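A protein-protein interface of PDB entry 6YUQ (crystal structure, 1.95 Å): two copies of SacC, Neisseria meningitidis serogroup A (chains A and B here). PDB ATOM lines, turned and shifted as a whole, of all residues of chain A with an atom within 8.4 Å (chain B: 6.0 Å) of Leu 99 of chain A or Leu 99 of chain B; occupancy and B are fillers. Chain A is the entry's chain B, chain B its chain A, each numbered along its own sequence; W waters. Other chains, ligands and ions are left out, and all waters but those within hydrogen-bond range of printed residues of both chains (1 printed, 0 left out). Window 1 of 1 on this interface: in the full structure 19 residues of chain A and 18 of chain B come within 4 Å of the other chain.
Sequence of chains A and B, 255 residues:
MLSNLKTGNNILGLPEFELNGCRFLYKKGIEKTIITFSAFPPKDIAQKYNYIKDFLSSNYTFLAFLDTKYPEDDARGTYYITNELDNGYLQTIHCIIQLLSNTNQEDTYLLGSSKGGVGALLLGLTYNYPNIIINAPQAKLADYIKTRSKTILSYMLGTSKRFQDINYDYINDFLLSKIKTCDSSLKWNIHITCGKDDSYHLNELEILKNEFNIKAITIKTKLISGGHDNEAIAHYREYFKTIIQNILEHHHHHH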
ATOM      1  N   MET A   1      -6.601  28.166 -20.874  1.00  0.00           N
ATOM      2  CA  MET A   1      -5.706  27.092 -21.266  1.00  0.00           C
ATOM      3  C   MET A   1      -6.155  25.831 -20.550  1.00  0.00           C
ATOM      4  O   MET A   1      -6.412  25.866 -19.352  1.00  0.00           O
ATOM      5  CB  MET A   1      -4.256  27.422 -20.928  1.00  0.00           C
ATOM      6  CG  MET A   1      -3.278  26.417 -21.503  1.00  0.00           C
ATOM      7  SD  MET A   1      -1.573  26.961 -21.399  1.00  0.00           S
ATOM      8  CE  MET A   1      -1.444  27.267 -19.641  1.00  0.00           C
ATOM      9  N   LEU A   2      -6.258  24.732 -21.300  1.00  0.00           N
ATOM     10  CA  LEU A   2      -6.827  23.503 -20.753  1.00  0.00           C
ATOM     11  C   LEU A   2      -6.147  23.103 -19.448  1.00  0.00           C
ATOM     12  O   LEU A   2      -6.815  22.817 -18.447  1.00  0.00           O
ATOM     13  CB  LEU A   2      -6.722  22.380 -21.784  1.00  0.00           C
ATOM     14  CG  LEU A   2      -7.116  20.982 -21.306  1.00  0.00           C
ATOM     15  CD1 LEU A   2      -8.582  20.952 -20.892  1.00  0.00           C
ATOM     16  CD2 LEU A   2      -6.844  19.961 -22.402  1.00  0.00           C
ATOM     17  N   SER A   3      -4.812  23.113 -19.432  1.00  0.00           N
ATOM     18  CA  SER A   3      -4.082  22.629 -18.264  1.00  0.00           C
ATOM     19  C   SER A   3      -4.353  23.479 -17.030  1.00  0.00           C
ATOM     20  O   SER A   3      -4.228  22.986 -15.903  1.00  0.00           O
ATOM     21  CB  SER A   3      -2.587  22.583 -18.561  1.00  0.00           C
ATOM     22  OG  SER A   3      -2.063  23.888 -18.703  1.00  0.00           O
ATOM     23  N   LEU A   5      -7.279  24.498 -16.250  1.00  0.00           N
ATOM     24  CA  LEU A   5      -8.588  24.103 -15.753  1.00  0.00           C
ATOM     25  C   LEU A   5      -8.532  22.889 -14.827  1.00  0.00           C
ATOM     26  O   LEU A   5      -9.587  22.373 -14.447  1.00  0.00           O
ATOM     27  CB  LEU A   5      -9.524  23.799 -16.928  1.00  0.00           C
ATOM     28  CG  LEU A   5      -9.594  24.904 -17.975  1.00  0.00           C
ATOM     29  CD1 LEU A   5     -10.498  24.495 -19.127  1.00  0.00           C
ATOM     30  CD2 LEU A   5     -10.085  26.173 -17.311  1.00  0.00           C
ATOM     31  N   PHE A  17     -10.474  17.994 -15.173  1.00  0.00           N
ATOM     32  CA  PHE A  17     -10.628  19.393 -15.549  1.00  0.00           C
ATOM     33  C   PHE A  17     -11.995  19.907 -15.113  1.00  0.00           C
ATOM     34  O   PHE A  17     -12.938  19.134 -14.911  1.00  0.00           O
ATOM     35  CB  PHE A  17     -10.503  19.578 -17.065  1.00  0.00           C
ATOM     36  CG  PHE A  17      -9.227  19.057 -17.642  1.00  0.00           C
ATOM     37  CD1 PHE A  17      -8.069  19.808 -17.571  1.00  0.00           C
ATOM     38  CD2 PHE A  17      -9.188  17.822 -18.270  1.00  0.00           C
ATOM     39  CE1 PHE A  17      -6.892  19.340 -18.110  1.00  0.00           C
ATOM     40  CE2 PHE A  17      -8.009  17.340 -18.810  1.00  0.00           C
ATOM     41  CZ  PHE A  17      -6.861  18.099 -18.730  1.00  0.00           C
ATOM     42  N   GLU A  18     -12.106  21.230 -15.010  1.00  0.00           N
ATOM     43  CA  GLU A  18     -13.399  21.850 -14.756  1.00  0.00           C
ATOM     44  C   GLU A  18     -13.489  23.170 -15.509  1.00  0.00           C
ATOM     45  O   GLU A  18     -12.580  24.004 -15.425  1.00  0.00           O
ATOM     46  CB  GLU A  18     -13.621  22.084 -13.260  1.00  0.00           C
ATOM     47  CG  GLU A  18     -15.019  22.586 -12.926  1.00  0.00           C
ATOM     48  CD  GLU A  18     -15.263  22.680 -11.435  1.00  0.00           C
ATOM     49  OE1 GLU A  18     -14.996  21.693 -10.724  1.00  0.00           O
ATOM     50  OE2 GLU A  18     -15.733  23.735 -10.970  1.00  0.00           O
ATOM     51  N   LEU A  19     -14.592  23.356 -16.234  1.00  0.00           N
ATOM     52  CA  LEU A  19     -14.838  24.579 -16.989  1.00  0.00           C
ATOM     53  C   LEU A  19     -16.285  24.992 -16.771  1.00  0.00           C
ATOM     54  O   LEU A  19     -17.202  24.248 -17.126  1.00  0.00           O
ATOM     55  CB  LEU A  19     -14.557  24.380 -18.485  1.00  0.00           C
ATOM     56  CG  LEU A  19     -14.887  25.558 -19.409  1.00  0.00           C
ATOM     57  CD1 LEU A  19     -13.973  26.733 -19.092  1.00  0.00           C
ATOM     58  CD2 LEU A  19     -14.760  25.164 -20.895  1.00  0.00           C
ATOM     59  N   PHE A  24     -14.757  17.270 -16.139  1.00  0.00           N
ATOM     60  CA  PHE A  24     -14.586  16.269 -17.184  1.00  0.00           C
ATOM     61  C   PHE A  24     -13.176  15.699 -17.180  1.00  0.00           C
ATOM     62  O   PHE A  24     -12.231  16.307 -16.669  1.00  0.00           O
ATOM     63  CB  PHE A  24     -14.934  16.828 -18.573  1.00  0.00           C
ATOM     64  CG  PHE A  24     -14.029  17.943 -19.049  1.00  0.00           C
ATOM     65  CD1 PHE A  24     -14.243  19.257 -18.649  1.00  0.00           C
ATOM     66  CD2 PHE A  24     -12.983  17.676 -19.920  1.00  0.00           C
ATOM     67  CE1 PHE A  24     -13.417  20.292 -19.114  1.00  0.00           C
ATOM     68  CE2 PHE A  24     -12.151  18.697 -20.380  1.00  0.00           C
ATOM     69  CZ  PHE A  24     -12.371  20.010 -19.975  1.00  0.00           C
ATOM     70  N   TYR A  26     -10.377  13.925 -20.038  1.00  0.00           N
ATOM     71  CA  TYR A  26     -10.075  14.022 -21.458  1.00  0.00           C
ATOM     72  C   TYR A  26      -8.795  13.270 -21.779  1.00  0.00           C
ATOM     73  O   TYR A  26      -7.755  13.510 -21.161  1.00  0.00           O
ATOM     74  CB  TYR A  26      -9.931  15.493 -21.874  1.00  0.00           C
ATOM     75  CG  TYR A  26      -9.448  15.733 -23.289  1.00  0.00           C
ATOM     76  CD1 TYR A  26     -10.102  15.179 -24.388  1.00  0.00           C
ATOM     77  CD2 TYR A  26      -8.348  16.547 -23.527  1.00  0.00           C
ATOM     78  CE1 TYR A  26      -9.664  15.428 -25.678  1.00  0.00           C
ATOM     79  CE2 TYR A  26      -7.909  16.805 -24.804  1.00  0.00           C
ATOM     80  CZ  TYR A  26      -8.563  16.249 -25.877  1.00  0.00           C
ATOM     81  OH  TYR A  26      -8.092  16.529 -27.141  1.00  0.00           O
ATOM     82  N   LYS A  28      -6.823  12.454 -25.456  1.00  0.00           N
ATOM     83  CA  LYS A  28      -6.828  12.629 -26.901  1.00  0.00           C
ATOM     84  C   LYS A  28      -6.417  11.333 -27.581  1.00  0.00           C
ATOM     85  O   LYS A  28      -5.421  10.711 -27.199  1.00  0.00           O
ATOM     86  CB  LYS A  28      -5.888  13.763 -27.311  1.00  0.00           C
ATOM     87  CG  LYS A  28      -5.999  14.170 -28.775  1.00  0.00           C
ATOM     88  CD  LYS A  28      -5.099  15.361 -29.082  1.00  0.00           C
ATOM     89  CE  LYS A  28      -5.419  15.983 -30.435  1.00  0.00           C
ATOM     90  NZ  LYS A  28      -4.871  17.372 -30.554  1.00  0.00           N
ATOM     91  N   LEU A  63     -13.801  11.451 -23.634  1.00  0.00           N
ATOM     92  CA  LEU A  63     -14.293  12.520 -22.771  1.00  0.00           C
ATOM     93  C   LEU A  63     -15.336  11.933 -21.835  1.00  0.00           C
ATOM     94  O   LEU A  63     -16.314  11.335 -22.296  1.00  0.00           O
ATOM     95  CB  LEU A  63     -14.910  13.659 -23.585  1.00  0.00           C
ATOM     96  CG  LEU A  63     -14.008  14.678 -24.275  1.00  0.00           C
ATOM     97  CD1 LEU A  63     -14.843  15.519 -25.210  1.00  0.00           C
ATOM     98  CD2 LEU A  63     -13.336  15.576 -23.257  1.00  0.00           C
ATOM     99  N   THR A  92     -22.227  24.074 -22.252  1.00  0.00           N
ATOM    100  CA  THR A  92     -20.822  23.951 -21.877  1.00  0.00           C
ATOM    101  C   THR A  92     -20.254  22.611 -22.341  1.00  0.00           C
ATOM    102  O   THR A  92     -19.169  22.554 -22.931  1.00  0.00           O
ATOM    103  CB  THR A  92     -20.665  24.112 -20.360  1.00  0.00           C
ATOM    104  OG1 THR A  92     -20.953  25.467 -19.982  1.00  0.00           O
ATOM    105  CG2 THR A  92     -19.249  23.764 -19.918  1.00  0.00           C
ATOM    106  N   ILE A  93     -20.983  21.517 -22.091  1.00  0.00           N
ATOM    107  CA  ILE A  93     -20.514  20.202 -22.528  1.00  0.00           C
ATOM    108  C   ILE A  93     -20.330  20.173 -24.043  1.00  0.00           C
ATOM    109  O   ILE A  93     -19.328  19.652 -24.549  1.00  0.00           O
ATOM    110  CB  ILE A  93     -21.480  19.103 -22.046  1.00  0.00           C
ATOM    111  CG1 ILE A  93     -21.438  18.972 -20.523  1.00  0.00           C
ATOM    112  CG2 ILE A  93     -21.130  17.760 -22.681  1.00  0.00           C
ATOM    113  CD1 ILE A  93     -22.453  17.962 -19.965  1.00  0.00           C
ATOM    114  N   HIS A  94     -21.276  20.762 -24.785  1.00  0.00           N
ATOM    115  CA  HIS A  94     -21.163  20.843 -26.241  1.00  0.00           C
ATOM    116  C   HIS A  94     -19.887  21.563 -26.675  1.00  0.00           C
ATOM    117  O   HIS A  94     -19.207  21.122 -27.609  1.00  0.00           O
ATOM    118  CB  HIS A  94     -22.392  21.553 -26.820  1.00  0.00           C
ATOM    119  CG  HIS A  94     -22.397  21.647 -28.318  1.00  0.00           C
ATOM    120  ND1 HIS A  94     -22.212  20.554 -29.134  1.00  0.00           N
ATOM    121  CD2 HIS A  94     -22.583  22.704 -29.146  1.00  0.00           C
ATOM    122  CE1 HIS A  94     -22.279  20.929 -30.396  1.00  0.00           C
ATOM    123  NE2 HIS A  94     -22.501  22.230 -30.433  1.00  0.00           N
ATOM    124  N   CYS A  95     -19.557  22.687 -26.025  1.00  0.00           N
ATOM    125  CA  CYS A  95     -18.382  23.458 -26.432  1.00  0.00           C
ATOM    126  C   CYS A  95     -17.095  22.697 -26.147  1.00  0.00           C
ATOM    127  O   CYS A  95     -16.134  22.771 -26.923  1.00  0.00           O
ATOM    128  CB  CYS A  95     -18.343  24.810 -25.707  1.00  0.00           C
ATOM    129  SG  CYS A  95     -19.641  25.989 -26.114  1.00  0.00           S
ATOM    130  N   ILE A  96     -17.043  22.022 -24.999  1.00  0.00           N
ATOM    131  CA  ILE A  96     -15.892  21.195 -24.645  1.00  0.00           C
ATOM    132  C   ILE A  96     -15.674  20.116 -25.703  1.00  0.00           C
ATOM    133  O   ILE A  96     -14.563  19.934 -26.211  1.00  0.00           O
ATOM    134  CB  ILE A  96     -16.098  20.587 -23.243  1.00  0.00           C
ATOM    135  CG1 ILE A  96     -16.048  21.674 -22.159  1.00  0.00           C
ATOM    136  CG2 ILE A  96     -15.070  19.518 -22.958  1.00  0.00           C
ATOM    137  CD1 ILE A  96     -16.584  21.206 -20.808  1.00  0.00           C
ATOM    138  N   ILE A  97     -16.744  19.403 -26.070  1.00  0.00           N
ATOM    139  CA  ILE A  97     -16.636  18.357 -27.087  1.00  0.00           C
ATOM    140  C   ILE A  97     -16.188  18.946 -28.419  1.00  0.00           C
ATOM    141  O   ILE A  97     -15.283  18.420 -29.072  1.00  0.00           O
ATOM    142  CB  ILE A  97     -17.969  17.595 -27.217  1.00  0.00           C
ATOM    143  CG1 ILE A  97     -18.288  16.876 -25.905  1.00  0.00           C
ATOM    144  CG2 ILE A  97     -17.914  16.581 -28.368  1.00  0.00           C
ATOM    145  CD1 ILE A  97     -19.593  16.110 -25.916  1.00  0.00           C
ATOM    146  N   GLN A  98     -16.797  20.063 -28.834  1.00  0.00           N
ATOM    147  CA  GLN A  98     -16.534  20.582 -30.174  1.00  0.00           C
ATOM    148  C   GLN A  98     -15.106  21.086 -30.323  1.00  0.00           C
ATOM    149  O   GLN A  98     -14.542  21.023 -31.419  1.00  0.00           O
ATOM    150  CB  GLN A  98     -17.517  21.705 -30.515  1.00  0.00           C
ATOM    151  CG  GLN A  98     -18.902  21.222 -30.890  1.00  0.00           C
ATOM    152  CD  GLN A  98     -18.873  20.132 -31.942  1.00  0.00           C
ATOM    153  OE1 GLN A  98     -18.375  20.336 -33.051  1.00  0.00           O
ATOM    154  NE2 GLN A  98     -19.407  18.960 -31.594  1.00  0.00           N
ATOM    155  N   LEU A  99     -14.512  21.600 -29.253  1.00  0.00           N
ATOM    156  CA  LEU A  99     -13.184  22.187 -29.350  1.00  0.00           C
ATOM    157  C   LEU A  99     -12.067  21.214 -29.001  1.00  0.00           C
ATOM    158  O   LEU A  99     -10.924  21.430 -29.420  1.00  0.00           O
ATOM    159  CB  LEU A  99     -13.088  23.409 -28.434  1.00  0.00           C
ATOM    160  CG  LEU A  99     -14.002  24.575 -28.803  1.00  0.00           C
ATOM    161  CD1 LEU A  99     -13.950  25.595 -27.678  1.00  0.00           C
ATOM    162  CD2 LEU A  99     -13.579  25.218 -30.135  1.00  0.00           C
ATOM    163  N   LEU A 100     -12.358  20.161 -28.235  1.00  0.00           N
ATOM    164  CA  LEU A 100     -11.337  19.188 -27.864  1.00  0.00           C
ATOM    165  C   LEU A 100     -11.390  17.913 -28.696  1.00  0.00           C
ATOM    166  O   LEU A 100     -10.386  17.195 -28.760  1.00  0.00           O
ATOM    167  CB  LEU A 100     -11.456  18.818 -26.376  1.00  0.00           C
ATOM    168  CG  LEU A 100     -11.201  19.932 -25.351  1.00  0.00           C
ATOM    169  CD1 LEU A 100     -11.261  19.394 -23.921  1.00  0.00           C
ATOM    170  CD2 LEU A 100      -9.870  20.606 -25.609  1.00  0.00           C
ATOM    171  N   SER A 101     -12.523  17.605 -29.318  1.00  0.00           N
ATOM    172  CA  SER A 101     -12.616  16.398 -30.125  1.00  0.00           C
ATOM    173  C   SER A 101     -11.974  16.620 -31.488  1.00  0.00           C
ATOM    174  O   SER A 101     -11.989  17.725 -32.036  1.00  0.00           O
ATOM    175  CB  SER A 101     -14.073  15.964 -30.290  1.00  0.00           C
ATOM    176  OG  SER A 101     -14.226  15.079 -31.383  1.00  0.00           O
ATOM    177  N   ASN A 102     -11.401  15.549 -32.036  1.00  0.00           N
ATOM    178  CA  ASN A 102     -10.726  15.603 -33.327  1.00  0.00           C
ATOM    179  C   ASN A 102     -11.368  14.659 -34.343  1.00  0.00           C
ATOM    180  O   ASN A 102     -10.682  14.105 -35.203  1.00  0.00           O
ATOM    181  CB  ASN A 102      -9.235  15.300 -33.170  1.00  0.00           C
ATOM    182  CG  ASN A 102      -8.972  13.992 -32.440  1.00  0.00           C
ATOM    183  OD1 ASN A 102      -9.818  13.502 -31.694  1.00  0.00           O
ATOM    184  ND2 ASN A 102      -7.786  13.426 -32.648  1.00  0.00           N
ATOM    185  N   TYR A 129     -25.989  15.142 -32.067  1.00  0.00           N
ATOM    186  CA  TYR A 129     -25.003  14.072 -31.994  1.00  0.00           C
ATOM    187  C   TYR A 129     -25.746  12.781 -32.315  1.00  0.00           C
ATOM    188  O   TYR A 129     -26.570  12.337 -31.500  1.00  0.00           O
ATOM    189  CB  TYR A 129     -24.374  13.994 -30.612  1.00  0.00           C
ATOM    190  CG  TYR A 129     -23.398  15.105 -30.262  1.00  0.00           C
ATOM    191  CD1 TYR A 129     -22.037  14.982 -30.529  1.00  0.00           C
ATOM    192  CD2 TYR A 129     -23.834  16.261 -29.627  1.00  0.00           C
ATOM    193  CE1 TYR A 129     -21.142  15.991 -30.192  1.00  0.00           C
ATOM    194  CE2 TYR A 129     -22.950  17.275 -29.292  1.00  0.00           C
ATOM    195  CZ  TYR A 129     -21.605  17.135 -29.573  1.00  0.00           C
ATOM    196  OH  TYR A 129     -20.732  18.147 -29.231  1.00  0.00           O
ATOM    197  N   MET B   1     -15.293  18.885 -34.280  1.00  0.00           N
ATOM    198  CA  MET B   1     -13.903  19.316 -34.224  1.00  0.00           C
ATOM    199  C   MET B   1     -13.789  20.729 -34.768  1.00  0.00           C
ATOM    200  O   MET B   1     -14.646  21.164 -35.524  1.00  0.00           O
ATOM    201  CB  MET B   1     -13.003  18.366 -35.016  1.00  0.00           C
ATOM    202  CG  MET B   1     -13.587  17.888 -36.324  1.00  0.00           C
ATOM    203  SD  MET B   1     -12.445  16.786 -37.205  1.00  0.00           S
ATOM    204  CE  MET B   1     -10.872  17.375 -36.571  1.00  0.00           C
ATOM    205  N   LEU B   2     -12.718  21.427 -34.378  1.00  0.00           N
ATOM    206  CA  LEU B   2     -12.557  22.834 -34.738  1.00  0.00           C
ATOM    207  C   LEU B   2     -12.573  23.036 -36.249  1.00  0.00           C
ATOM    208  O   LEU B   2     -13.136  24.021 -36.744  1.00  0.00           O
ATOM    209  CB  LEU B   2     -11.260  23.380 -34.146  1.00  0.00           C
ATOM    210  CG  LEU B   2     -10.976  24.855 -34.433  1.00  0.00           C
ATOM    211  CD1 LEU B   2     -12.189  25.694 -34.050  1.00  0.00           C
ATOM    212  CD2 LEU B   2      -9.743  25.329 -33.680  1.00  0.00           C
ATOM    213  N   LEU B   5     -15.949  23.509 -37.645  1.00  0.00           N
ATOM    214  CA  LEU B   5     -16.666  24.729 -37.295  1.00  0.00           C
ATOM    215  C   LEU B   5     -16.420  25.862 -38.285  1.00  0.00           C
ATOM    216  O   LEU B   5     -16.931  26.969 -38.082  1.00  0.00           O
ATOM    217  CB  LEU B   5     -16.283  25.185 -35.883  1.00  0.00           C
ATOM    218  CG  LEU B   5     -16.401  24.142 -34.769  1.00  0.00           C
ATOM    219  CD1 LEU B   5     -15.795  24.671 -33.487  1.00  0.00           C
ATOM    220  CD2 LEU B   5     -17.849  23.749 -34.551  1.00  0.00           C
ATOM    221  N   LEU B  19     -19.340  28.672 -33.450  1.00  0.00           N
ATOM    222  CA  LEU B  19     -19.746  27.684 -32.455  1.00  0.00           C
ATOM    223  C   LEU B  19     -20.887  28.268 -31.644  1.00  0.00           C
ATOM    224  O   LEU B  19     -20.717  29.308 -30.999  1.00  0.00           O
ATOM    225  CB  LEU B  19     -18.582  27.301 -31.537  1.00  0.00           C
ATOM    226  CG  LEU B  19     -18.959  26.437 -30.330  1.00  0.00           C
ATOM    227  CD1 LEU B  19     -19.432  25.066 -30.783  1.00  0.00           C
ATOM    228  CD2 LEU B  19     -17.781  26.305 -29.376  1.00  0.00           C
ATOM    229  N   PHE B  24     -15.995  33.582 -34.819  1.00  0.00           N
ATOM    230  CA  PHE B  24     -14.691  34.019 -34.346  1.00  0.00           C
ATOM    231  C   PHE B  24     -13.596  33.616 -35.322  1.00  0.00           C
ATOM    232  O   PHE B  24     -13.747  32.683 -36.116  1.00  0.00           O
ATOM    233  CB  PHE B  24     -14.380  33.470 -32.940  1.00  0.00           C
ATOM    234  CG  PHE B  24     -14.226  31.970 -32.875  1.00  0.00           C
ATOM    235  CD1 PHE B  24     -15.334  31.149 -32.692  1.00  0.00           C
ATOM    236  CD2 PHE B  24     -12.973  31.385 -32.959  1.00  0.00           C
ATOM    237  CE1 PHE B  24     -15.197  29.769 -32.611  1.00  0.00           C
ATOM    238  CE2 PHE B  24     -12.823  29.997 -32.879  1.00  0.00           C
ATOM    239  CZ  PHE B  24     -13.936  29.188 -32.706  1.00  0.00           C
ATOM    240  N   HIS B  94     -16.183  32.486 -23.386  1.00  0.00           N
ATOM    241  CA  HIS B  94     -15.278  31.994 -22.345  1.00  0.00           C
ATOM    242  C   HIS B  94     -14.784  30.581 -22.653  1.00  0.00           C
ATOM    243  O   HIS B  94     -13.584  30.298 -22.558  1.00  0.00           O
ATOM    244  CB  HIS B  94     -15.993  32.044 -20.987  1.00  0.00           C
ATOM    245  CG  HIS B  94     -15.143  31.626 -19.824  1.00  0.00           C
ATOM    246  ND1 HIS B  94     -13.935  32.219 -19.535  1.00  0.00           N
ATOM    247  CD2 HIS B  94     -15.329  30.673 -18.878  1.00  0.00           C
ATOM    248  CE1 HIS B  94     -13.415  31.660 -18.458  1.00  0.00           C
ATOM    249  NE2 HIS B  94     -14.240  30.715 -18.040  1.00  0.00           N
ATOM    250  N   CYS B  95     -15.693  29.673 -23.020  1.00  0.00           N
ATOM    251  CA  CYS B  95     -15.266  28.308 -23.326  1.00  0.00           C
ATOM    252  C   CYS B  95     -14.271  28.276 -24.484  1.00  0.00           C
ATOM    253  O   CYS B  95     -13.278  27.538 -24.440  1.00  0.00           O
ATOM    254  CB  CYS B  95     -16.476  27.432 -23.641  1.00  0.00           C
ATOM    255  SG  CYS B  95     -17.525  27.138 -22.206  1.00  0.00           S
ATOM    256  N   ILE B  96     -14.523  29.073 -25.525  1.00  0.00           N
ATOM    257  CA  ILE B  96     -13.637  29.098 -26.688  1.00  0.00           C
ATOM    258  C   ILE B  96     -12.232  29.526 -26.276  1.00  0.00           C
ATOM    259  O   ILE B  96     -11.239  28.865 -26.610  1.00  0.00           O
ATOM    260  CB  ILE B  96     -14.222  30.026 -27.775  1.00  0.00           C
ATOM    261  CG1 ILE B  96     -15.497  29.408 -28.362  1.00  0.00           C
ATOM    262  CG2 ILE B  96     -13.187  30.321 -28.872  1.00  0.00           C
ATOM    263  CD1 ILE B  96     -16.360  30.355 -29.169  1.00  0.00           C
ATOM    264  N   ILE B  97     -12.134  30.626 -25.521  1.00  0.00           N
ATOM    265  CA  ILE B  97     -10.834  31.142 -25.087  1.00  0.00           C
ATOM    266  C   ILE B  97     -10.121  30.139 -24.186  1.00  0.00           C
ATOM    267  O   ILE B  97      -8.927  29.861 -24.356  1.00  0.00           O
ATOM    268  CB  ILE B  97     -11.013  32.492 -24.376  1.00  0.00           C
ATOM    269  CG1 ILE B  97     -11.628  33.515 -25.335  1.00  0.00           C
ATOM    270  CG2 ILE B  97      -9.666  32.997 -23.846  1.00  0.00           C
ATOM    271  CD1 ILE B  97     -12.136  34.771 -24.642  1.00  0.00           C
ATOM    272  N   GLN B  98     -10.835  29.589 -23.205  1.00  0.00           N
ATOM    273  CA  GLN B  98     -10.178  28.729 -22.231  1.00  0.00           C
ATOM    274  C   GLN B  98      -9.624  27.470 -22.874  1.00  0.00           C
ATOM    275  O   GLN B  98      -8.598  26.950 -22.426  1.00  0.00           O
ATOM    276  CB  GLN B  98     -11.150  28.389 -21.108  1.00  0.00           C
ATOM    277  CG  GLN B  98     -11.438  29.607 -20.236  1.00  0.00           C
ATOM    278  CD  GLN B  98     -10.181  30.167 -19.602  1.00  0.00           C
ATOM    279  OE1 GLN B  98      -9.492  29.469 -18.852  1.00  0.00           O
ATOM    280  NE2 GLN B  98      -9.878  31.434 -19.888  1.00  0.00           N
ATOM    281  N   LEU B  99     -10.262  26.975 -23.930  1.00  0.00           N
ATOM    282  CA  LEU B  99      -9.813  25.726 -24.529  1.00  0.00           C
ATOM    283  C   LEU B  99      -8.826  25.932 -25.670  1.00  0.00           C
ATOM    284  O   LEU B  99      -7.929  25.100 -25.864  1.00  0.00           O
ATOM    285  CB  LEU B  99     -11.017  24.923 -25.025  1.00  0.00           C
ATOM    286  CG  LEU B  99     -11.943  24.471 -23.899  1.00  0.00           C
ATOM    287  CD1 LEU B  99     -13.235  23.911 -24.477  1.00  0.00           C
ATOM    288  CD2 LEU B  99     -11.233  23.423 -23.055  1.00  0.00           C
ATOM    289  N   LEU B 100      -8.970  27.013 -26.428  1.00  0.00           N
ATOM    290  CA  LEU B 100      -8.079  27.277 -27.550  1.00  0.00           C
ATOM    291  C   LEU B 100      -6.823  28.050 -27.168  1.00  0.00           C
ATOM    292  O   LEU B 100      -5.820  27.950 -27.880  1.00  0.00           O
ATOM    293  CB  LEU B 100      -8.828  28.042 -28.645  1.00  0.00           C
ATOM    294  CG  LEU B 100      -9.949  27.279 -29.361  1.00  0.00           C
ATOM    295  CD1 LEU B 100     -10.365  28.004 -30.647  1.00  0.00           C
ATOM    296  CD2 LEU B 100      -9.546  25.822 -29.642  1.00  0.00           C
ATOM    297  N   SER B 101      -6.839  28.819 -26.079  1.00  0.00           N
ATOM    298  CA  SER B 101      -5.658  29.596 -25.721  1.00  0.00           C
ATOM    299  C   SER B 101      -4.543  28.698 -25.183  1.00  0.00           C
ATOM    300  O   SER B 101      -4.790  27.653 -24.574  1.00  0.00           O
ATOM    301  CB  SER B 101      -6.012  30.671 -24.691  1.00  0.00           C
ATOM    302  OG  SER B 101      -4.896  30.974 -23.874  1.00  0.00           O
HETATM  303  O   HOH W   1      -5.841  25.002 -24.177  1.00  0.00           O
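Met 1 of chain A touches Ser 101 of chain B, and with the chains exchanged Ser 101 of chain A touches Met 1 of chain B.
Leu 19 of chain A touches Cys 95 of chain B, and with the chains exchanged Cys 95 of chain A touches Leu 19 of chain B.
Leu 19 of chain A touches Gln 98 of chain B, and with the chains exchanged Gln 98 of chain A touches Leu 19 of chain B.
Of the 19 pairs that touch across the chains among the printed residues, 18 have their exchanged pair printed and touching as well.
N of Glu 18 of chain A is in hydrogen-bond range of O of Leu 5 of chain A, at 2.8 Å.
The side-chain hydroxyl (OH) of Tyr 129 of chain A lies within hydrogen-bond range of the side-chain amide nitrogen (NE2) of Gln 98 of chain A, at 2.8 Å.
Water W1 lies within hydrogen-bond range of the backbone carbonyl oxygen (O) of Leu 99 of chain B, the backbone carbonyl oxygen (O) of Ser 101 of chain B and the backbone NH (N) of Leu 2 of chain A.
Met 1 of chain A touches Ser 101 of chain B.
Gln 98 of chain B touches Leu 5 of chain A (OE1 to CD2, 3.7 Å).
Leu 19 of chain A touches Cys 95 of chain B.
CD1 of Leu 99 of chain B touches O of Cys 95 of chain A, 3.96 Å away.
Met 1 of chain B touches Gln 98 of chain A (CA to O, 3.3 Å).
Leu 5 of chain B touches Gln 98 of chain A.
CD1 of Leu 99 of chain A touches CA of Ile 96 of chain B, at 3.7 Å.
Met 1 of chain B touches Ser 101 of chain A.
N of Leu 2 of chain B is in hydrogen-bond range of O of Gln 98 of chain A, 3.5 Å away.
The backbone NH (N) of Met 1 of chain A lies within hydrogen-bond range of the backbone carbonyl oxygen (O) of Gln 98 of chain B.
The backbone carbonyl oxygen of Gln 98 of chain B lies within hydrogen-bond range of the backbone NH of Leu 2 of chain A, at 3.4 Å.
SD of Met 1 of chain B sits close to O of Asn 102 of chain A (3.8 Å).
Of the 23 printed residues of chain A, 10 touch a printed residue of chain B.
Of the 13 printed residues of chain B, 9 touch a printed residue of chain A.
Hydrophobic or aromatic side chains of chain B that line the printed part of chain A: Met 1, Leu 5, Leu 19 and Leu 99.
Among the printed residues, no Asp or Glu carboxylate lies within 4 Å of a Lys or Arg side-chain nitrogen of the other chain.
Leu 99 of chain A touches three residues of chain B.
Leu 99 of chain B touches three residues of chain A.
Of the printed residues of chain B, Cys 95 of chain A touches Leu 19 (3.8 Å), Cys 95 (3.8 Å) and Leu 99 (3.96 Å).
Of the printed residues of chain A, Leu 5 of chain B touches Gln 98.
Printed residues of chain A within 4 Å of Met 1 of chain B: Gln 98, Ser 101 and Asn 102.
Of the printed residues of chain A, Cys 95 of chain B touches Leu 19 (3.6 Å), Cys 95 (3.8 Å) and Leu 99 (3.8 Å).
Leu 63 of chain A touches none of the printed residues of chain B.
The nearest residue of chain B that does not touch Leu 99 of chain A is Leu 5 of chain B (4.1 Å).
The nearest printed residue of chain B that does not touch Cys 95 of chain A is Ile 96 of chain B (5.7 Å).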
